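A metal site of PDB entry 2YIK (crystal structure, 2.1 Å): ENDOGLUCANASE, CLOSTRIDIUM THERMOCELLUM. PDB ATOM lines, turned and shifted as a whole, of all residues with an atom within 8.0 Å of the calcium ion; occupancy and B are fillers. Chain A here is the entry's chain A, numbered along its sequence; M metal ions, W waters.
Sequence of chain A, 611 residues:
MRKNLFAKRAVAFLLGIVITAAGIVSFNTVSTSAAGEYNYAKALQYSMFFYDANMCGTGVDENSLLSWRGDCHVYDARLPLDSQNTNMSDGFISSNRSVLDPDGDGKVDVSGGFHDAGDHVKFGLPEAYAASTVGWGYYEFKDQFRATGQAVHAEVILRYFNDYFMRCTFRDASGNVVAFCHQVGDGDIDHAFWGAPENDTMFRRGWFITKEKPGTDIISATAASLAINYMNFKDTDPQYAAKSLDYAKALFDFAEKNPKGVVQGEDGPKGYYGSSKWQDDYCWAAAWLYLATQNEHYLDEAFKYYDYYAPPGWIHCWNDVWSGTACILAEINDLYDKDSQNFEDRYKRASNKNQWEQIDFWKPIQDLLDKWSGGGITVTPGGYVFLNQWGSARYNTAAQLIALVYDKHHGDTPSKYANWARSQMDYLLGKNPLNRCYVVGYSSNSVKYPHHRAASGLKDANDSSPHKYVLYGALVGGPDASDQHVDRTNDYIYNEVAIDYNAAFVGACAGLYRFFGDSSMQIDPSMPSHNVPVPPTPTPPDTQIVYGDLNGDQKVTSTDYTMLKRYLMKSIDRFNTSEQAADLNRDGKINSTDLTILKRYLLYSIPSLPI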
ATOM      1  N   LEU A 125       3.033  37.846  -7.524  1.00  0.00           N
ATOM      2  CA  LEU A 125       2.722  36.526  -8.047  1.00  0.00           C
ATOM      3  C   LEU A 125       3.015  36.424  -9.540  1.00  0.00           C
ATOM      4  O   LEU A 125       3.747  35.526  -9.960  1.00  0.00           O
ATOM      5  CB  LEU A 125       1.275  36.129  -7.740  1.00  0.00           C
ATOM      6  CG  LEU A 125       0.908  34.653  -7.900  1.00  0.00           C
ATOM      7  CD1 LEU A 125       2.015  33.769  -7.326  1.00  0.00           C
ATOM      8  CD2 LEU A 125      -0.417  34.380  -7.194  1.00  0.00           C
ATOM      9  N   THR A 216       3.043  32.355   1.575  1.00  0.00           N
ATOM     10  CA  THR A 216       3.625  31.162   0.978  1.00  0.00           C
ATOM     11  C   THR A 216       3.632  31.092  -0.544  1.00  0.00           C
ATOM     12  O   THR A 216       4.627  30.706  -1.138  1.00  0.00           O
ATOM     13  CB  THR A 216       2.922  29.918   1.522  1.00  0.00           C
ATOM     14  OG1 THR A 216       2.667  30.112   2.925  1.00  0.00           O
ATOM     15  CG2 THR A 216       3.786  28.677   1.330  1.00  0.00           C
ATOM     16  N   ASP A 217       2.522  31.458  -1.180  1.00  0.00           N
ATOM     17  CA  ASP A 217       2.470  31.389  -2.628  1.00  0.00           C
ATOM     18  C   ASP A 217       3.514  32.291  -3.299  1.00  0.00           C
ATOM     19  O   ASP A 217       4.284  31.820  -4.134  1.00  0.00           O
ATOM     20  CB  ASP A 217       1.050  31.696  -3.134  1.00  0.00           C
ATOM     21  CG  ASP A 217       0.568  33.079  -2.740  1.00  0.00           C
ATOM     22  OD1 ASP A 217       0.957  33.564  -1.651  1.00  0.00           O
ATOM     23  OD2 ASP A 217      -0.225  33.674  -3.513  1.00  0.00           O
ATOM     24  N   ILE A 218       3.544  33.568  -2.937  1.00  0.00           N
ATOM     25  CA  ILE A 218       4.515  34.491  -3.541  1.00  0.00           C
ATOM     26  C   ILE A 218       5.959  34.184  -3.138  1.00  0.00           C
ATOM     27  O   ILE A 218       6.860  34.272  -3.966  1.00  0.00           O
ATOM     28  CB  ILE A 218       4.214  35.977  -3.189  1.00  0.00           C
ATOM     29  CG1 ILE A 218       2.953  36.460  -3.917  1.00  0.00           C
ATOM     30  CG2 ILE A 218       5.376  36.856  -3.611  1.00  0.00           C
ATOM     31  CD1 ILE A 218       1.695  35.947  -3.298  1.00  0.00           C
ATOM     32  N   ALA A 221       6.916  31.148  -5.184  1.00  0.00           N
ATOM     33  CA  ALA A 221       7.011  31.477  -6.603  1.00  0.00           C
ATOM     34  C   ALA A 221       8.325  32.176  -6.853  1.00  0.00           C
ATOM     35  O   ALA A 221       8.997  31.914  -7.852  1.00  0.00           O
ATOM     36  CB  ALA A 221       5.843  32.368  -7.022  1.00  0.00           C
ATOM     37  N   VAL A 262      -1.971  32.086   1.375  1.00  0.00           N
ATOM     38  CA  VAL A 262      -1.642  32.911   0.225  1.00  0.00           C
ATOM     39  C   VAL A 262      -1.726  34.381   0.629  1.00  0.00           C
ATOM     40  O   VAL A 262      -2.418  34.731   1.584  1.00  0.00           O
ATOM     41  CB  VAL A 262      -2.616  32.665  -0.963  1.00  0.00           C
ATOM     42  CG1 VAL A 262      -2.566  31.190  -1.375  1.00  0.00           C
ATOM     43  CG2 VAL A 262      -4.042  33.071  -0.585  1.00  0.00           C
ATOM     44  N   GLY A 274      -5.915  37.522  -7.686  1.00  0.00           N
ATOM     45  CA  GLY A 274      -6.442  36.696  -6.609  1.00  0.00           C
ATOM     46  C   GLY A 274      -5.827  35.323  -6.682  1.00  0.00           C
ATOM     47  O   GLY A 274      -6.055  34.584  -7.642  1.00  0.00           O
ATOM     48  N   SER A 275      -5.070  34.964  -5.663  1.00  0.00           N
ATOM     49  CA  SER A 275      -4.376  33.672  -5.614  1.00  0.00           C
ATOM     50  C   SER A 275      -5.213  32.527  -5.065  1.00  0.00           C
ATOM     51  O   SER A 275      -5.742  32.616  -3.961  1.00  0.00           O
ATOM     52  CB  SER A 275      -3.095  33.814  -4.778  1.00  0.00           C
ATOM     53  OG  SER A 275      -2.364  32.607  -4.733  1.00  0.00           O
ATOM     54  N   SER A 276      -5.305  31.441  -5.841  1.00  0.00           N
ATOM     55  CA  SER A 276      -6.079  30.271  -5.420  1.00  0.00           C
ATOM     56  C   SER A 276      -5.376  29.457  -4.336  1.00  0.00           C
ATOM     57  O   SER A 276      -5.990  29.090  -3.340  1.00  0.00           O
ATOM     58  CB  SER A 276      -6.348  29.366  -6.620  1.00  0.00           C
ATOM     59  OG  SER A 276      -7.095  30.064  -7.597  1.00  0.00           O
ATOM     60  N   LYS A 277      -4.087  29.156  -4.527  1.00  0.00           N
ATOM     61  CA  LYS A 277      -3.379  28.371  -3.533  1.00  0.00           C
ATOM     62  C   LYS A 277      -1.867  28.553  -3.532  1.00  0.00           C
ATOM     63  O   LYS A 277      -1.297  29.159  -4.428  1.00  0.00           O
ATOM     64  CB  LYS A 277      -3.688  26.887  -3.682  1.00  0.00           C
ATOM     65  CG  LYS A 277      -3.138  26.281  -4.953  1.00  0.00           C
ATOM     66  CD  LYS A 277      -3.979  26.688  -6.152  1.00  0.00           C
ATOM     67  CE  LYS A 277      -3.170  26.735  -7.456  1.00  0.00           C
ATOM     68  NZ  LYS A 277      -3.400  25.563  -8.359  1.00  0.00           N
ATOM     69  N   TRP A 278      -1.238  27.995  -2.513  1.00  0.00           N
ATOM     70  CA  TRP A 278       0.204  28.087  -2.363  1.00  0.00           C
ATOM     71  C   TRP A 278       0.922  26.763  -2.625  1.00  0.00           C
ATOM     72  O   TRP A 278       2.120  26.753  -2.904  1.00  0.00           O
ATOM     73  CB  TRP A 278       0.554  28.550  -0.942  1.00  0.00           C
ATOM     74  CG  TRP A 278       0.068  27.615   0.131  1.00  0.00           C
ATOM     75  CD1 TRP A 278      -1.112  27.713   0.839  1.00  0.00           C
ATOM     76  CD2 TRP A 278       0.730  26.442   0.631  1.00  0.00           C
ATOM     77  NE1 TRP A 278      -1.203  26.681   1.739  1.00  0.00           N
ATOM     78  CE2 TRP A 278      -0.092  25.899   1.648  1.00  0.00           C
ATOM     79  CE3 TRP A 278       1.947  25.815   0.327  1.00  0.00           C
ATOM     80  CZ2 TRP A 278       0.262  24.732   2.337  1.00  0.00           C
ATOM     81  CZ3 TRP A 278       2.298  24.646   1.030  1.00  0.00           C
ATOM     82  CH2 TRP A 278       1.451  24.129   2.037  1.00  0.00           C
ATOM     83  N   GLN A 279       0.200  25.654  -2.536  1.00  0.00           N
ATOM     84  CA  GLN A 279       0.814  24.340  -2.718  1.00  0.00           C
ATOM     85  C   GLN A 279       1.525  24.100  -4.049  1.00  0.00           C
ATOM     86  O   GLN A 279       2.552  23.436  -4.078  1.00  0.00           O
ATOM     87  CB  GLN A 279      -0.192  23.223  -2.436  1.00  0.00           C
ATOM     88  CG  GLN A 279      -0.610  23.154  -0.969  1.00  0.00           C
ATOM     89  CD  GLN A 279      -1.852  23.964  -0.670  1.00  0.00           C
ATOM     90  OE1 GLN A 279      -2.128  24.990  -1.301  1.00  0.00           O
ATOM     91  NE2 GLN A 279      -2.623  23.507   0.309  1.00  0.00           N
ATOM     92  N   ASP A 280       0.980  24.624  -5.147  1.00  0.00           N
ATOM     93  CA  ASP A 280       1.628  24.429  -6.442  1.00  0.00           C
ATOM     94  C   ASP A 280       2.933  25.227  -6.507  1.00  0.00           C
ATOM     95  O   ASP A 280       3.941  24.704  -6.976  1.00  0.00           O
ATOM     96  CB  ASP A 280       0.686  24.848  -7.574  1.00  0.00           C
ATOM     97  CG  ASP A 280       0.177  26.250  -7.410  1.00  0.00           C
ATOM     98  OD1 ASP A 280      -0.255  26.573  -6.293  1.00  0.00           O
ATOM     99  OD2 ASP A 280       0.207  27.014  -8.398  1.00  0.00           O
ATOM    100  N   ASP A 281       2.922  26.481  -6.055  1.00  0.00           N
ATOM    101  CA  ASP A 281       4.136  27.302  -6.079  1.00  0.00           C
ATOM    102  C   ASP A 281       5.198  26.680  -5.163  1.00  0.00           C
ATOM    103  O   ASP A 281       6.394  26.688  -5.470  1.00  0.00           O
ATOM    104  CB  ASP A 281       3.854  28.713  -5.587  1.00  0.00           C
ATOM    105  CG  ASP A 281       2.700  29.371  -6.314  1.00  0.00           C
ATOM    106  OD1 ASP A 281       2.835  29.720  -7.504  1.00  0.00           O
ATOM    107  OD2 ASP A 281       1.651  29.544  -5.670  1.00  0.00           O
ATOM    108  N   TYR A 282       4.748  26.177  -4.017  1.00  0.00           N
ATOM    109  CA  TYR A 282       5.639  25.555  -3.037  1.00  0.00           C
ATOM    110  C   TYR A 282       6.323  24.345  -3.679  1.00  0.00           C
ATOM    111  O   TYR A 282       7.545  24.209  -3.604  1.00  0.00           O
ATOM    112  CB  TYR A 282       4.819  25.123  -1.810  1.00  0.00           C
ATOM    113  CG  TYR A 282       5.650  24.678  -0.625  1.00  0.00           C
ATOM    114  CD1 TYR A 282       6.247  25.614   0.229  1.00  0.00           C
ATOM    115  CD2 TYR A 282       5.846  23.331  -0.356  1.00  0.00           C
ATOM    116  CE1 TYR A 282       7.025  25.207   1.312  1.00  0.00           C
ATOM    117  CE2 TYR A 282       6.615  22.906   0.724  1.00  0.00           C
ATOM    118  CZ  TYR A 282       7.203  23.850   1.561  1.00  0.00           C
ATOM    119  OH  TYR A 282       7.991  23.435   2.609  1.00  0.00           O
ATOM    120  N   CYS A 317       0.134  28.655 -15.535  1.00  0.00           N
ATOM    121  CA  CYS A 317      -0.187  30.093 -15.529  1.00  0.00           C
ATOM    122  C   CYS A 317       0.126  30.700 -14.164  1.00  0.00           C
ATOM    123  O   CYS A 317       0.332  29.963 -13.201  1.00  0.00           O
ATOM    124  CB  CYS A 317      -1.655  30.341 -15.871  1.00  0.00           C
ATOM    125  SG  CYS A 317      -2.814  29.611 -14.709  1.00  0.00           S
ATOM    126  N   TRP A 318       0.152  32.028 -14.067  1.00  0.00           N
ATOM    127  CA  TRP A 318       0.488  32.666 -12.788  1.00  0.00           C
ATOM    128  C   TRP A 318      -0.319  32.156 -11.597  1.00  0.00           C
ATOM    129  O   TRP A 318       0.193  32.143 -10.481  1.00  0.00           O
ATOM    130  CB  TRP A 318       0.361  34.200 -12.875  1.00  0.00           C
ATOM    131  CG  TRP A 318      -1.042  34.737 -13.030  1.00  0.00           C
ATOM    132  CD1 TRP A 318      -1.633  35.159 -14.179  1.00  0.00           C
ATOM    133  CD2 TRP A 318      -2.009  34.914 -11.974  1.00  0.00           C
ATOM    134  NE1 TRP A 318      -2.913  35.577 -13.921  1.00  0.00           N
ATOM    135  CE2 TRP A 318      -3.180  35.412 -12.607  1.00  0.00           C
ATOM    136  CE3 TRP A 318      -2.023  34.648 -10.609  1.00  0.00           C
ATOM    137  CZ2 TRP A 318      -4.339  35.729 -11.861  1.00  0.00           C
ATOM    138  CZ3 TRP A 318      -3.175  34.956  -9.884  1.00  0.00           C
ATOM    139  CH2 TRP A 318      -4.330  35.456 -10.514  1.00  0.00           C
ATOM    140  N   ASN A 319      -1.551  31.738 -11.813  1.00  0.00           N
ATOM    141  CA  ASN A 319      -2.390  31.263 -10.712  1.00  0.00           C
ATOM    142  C   ASN A 319      -2.417  29.732 -10.557  1.00  0.00           C
ATOM    143  O   ASN A 319      -3.174  29.184  -9.760  1.00  0.00           O
ATOM    144  CB  ASN A 319      -3.814  31.802 -10.879  1.00  0.00           C
ATOM    145  CG  ASN A 319      -4.628  31.706  -9.596  1.00  0.00           C
ATOM    146  OD1 ASN A 319      -4.108  31.920  -8.495  1.00  0.00           O
ATOM    147  ND2 ASN A 319      -5.919  31.414  -9.737  1.00  0.00           N
ATOM    148  N   ASP A 320      -1.572  29.039 -11.322  1.00  0.00           N
ATOM    149  CA  ASP A 320      -1.510  27.581 -11.234  1.00  0.00           C
ATOM    150  C   ASP A 320      -0.298  27.030 -11.967  1.00  0.00           C
ATOM    151  O   ASP A 320      -0.274  26.942 -13.189  1.00  0.00           O
ATOM    152  CB  ASP A 320      -2.761  26.951 -11.829  1.00  0.00           C
ATOM    153  CG  ASP A 320      -2.844  25.455 -11.558  1.00  0.00           C
ATOM    154  OD1 ASP A 320      -1.780  24.785 -11.537  1.00  0.00           O
ATOM    155  OD2 ASP A 320      -3.953  24.944 -11.373  1.00  0.00           O
ATOM    156  N   VAL A 321       0.720  26.647 -11.208  1.00  0.00           N
ATOM    157  CA  VAL A 321       1.935  26.111 -11.808  1.00  0.00           C
ATOM    158  C   VAL A 321       2.095  24.606 -11.572  1.00  0.00           C
ATOM    159  O   VAL A 321       3.206  24.079 -11.582  1.00  0.00           O
ATOM    160  CB  VAL A 321       3.181  26.882 -11.277  1.00  0.00           C
ATOM    161  CG1 VAL A 321       3.096  28.348 -11.704  1.00  0.00           C
ATOM    162  CG2 VAL A 321       3.273  26.763  -9.734  1.00  0.00           C
ATOM    163  N   TRP A 322       0.978  23.915 -11.374  1.00  0.00           N
ATOM    164  CA  TRP A 322       1.012  22.468 -11.174  1.00  0.00           C
ATOM    165  C   TRP A 322       1.570  21.722 -12.394  1.00  0.00           C
ATOM    166  O   TRP A 322       2.343  20.779 -12.249  1.00  0.00           O
ATOM    167  CB  TRP A 322      -0.386  21.921 -10.859  1.00  0.00           C
ATOM    168  CG  TRP A 322      -0.838  22.030  -9.407  1.00  0.00           C
ATOM    169  CD1 TRP A 322      -2.016  22.561  -8.960  1.00  0.00           C
ATOM    170  CD2 TRP A 322      -0.135  21.550  -8.240  1.00  0.00           C
ATOM    171  NE1 TRP A 322      -2.090  22.459  -7.589  1.00  0.00           N
ATOM    172  CE2 TRP A 322      -0.957  21.869  -7.120  1.00  0.00           C
ATOM    173  CE3 TRP A 322       1.103  20.946  -8.034  1.00  0.00           C
ATOM    174  CZ2 TRP A 322      -0.582  21.528  -5.811  1.00  0.00           C
ATOM    175  CZ3 TRP A 322       1.470  20.607  -6.719  1.00  0.00           C
ATOM    176  CH2 TRP A 322       0.643  20.923  -5.623  1.00  0.00           C
HETATM  177 CA    CA M   1      -0.627  29.064  -6.822  1.00  0.00          CA
HETATM  178  O   HOH W   1      -2.288  31.051  -6.759  1.00  0.00           O
HETATM  179  O   HOH W   2       0.550  30.263  -8.798  1.00  0.00           O
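The side-chain carboxylate (OD2) of Asp 280 sits close to the backbone NH (N) of Val 321 (2.9 Å).
NZ of Lys 277 is in salt-bridge range of OD2 of Asp 320, at 3.1 Å.
O of Gly 274 lies close to OD1 of Asn 319, at 3.4 Å.
OG of Ser 276 is in hydrogen-bond range of ND2 of Asn 319, 2.8 Å away.
Water W1 lies within hydrogen-bond range of OG of Ser 275, OD1 of Asn 319, N of Ser 276 and N of Lys 277.
Water W2 lies within hydrogen-bond range of the backbone carbonyl oxygen of Trp 318 (2.5 Å) and the side-chain carboxylate of Asp 281 (2.7 Å).
The calcium ion is bound by O of Lys 277 (2.5 Å), OD1 of Asp 280 (2.6 Å), water W1 (2.6 Å), water W2 (2.6 Å), OD2 of Asp 281 (2.6 Å) and OD2 of Asp 280 (2.7 Å).
The calcium ion has six donor atoms within binding distance.
Residues that only touch the calcium ion: Asn 319 (3.9 Å).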
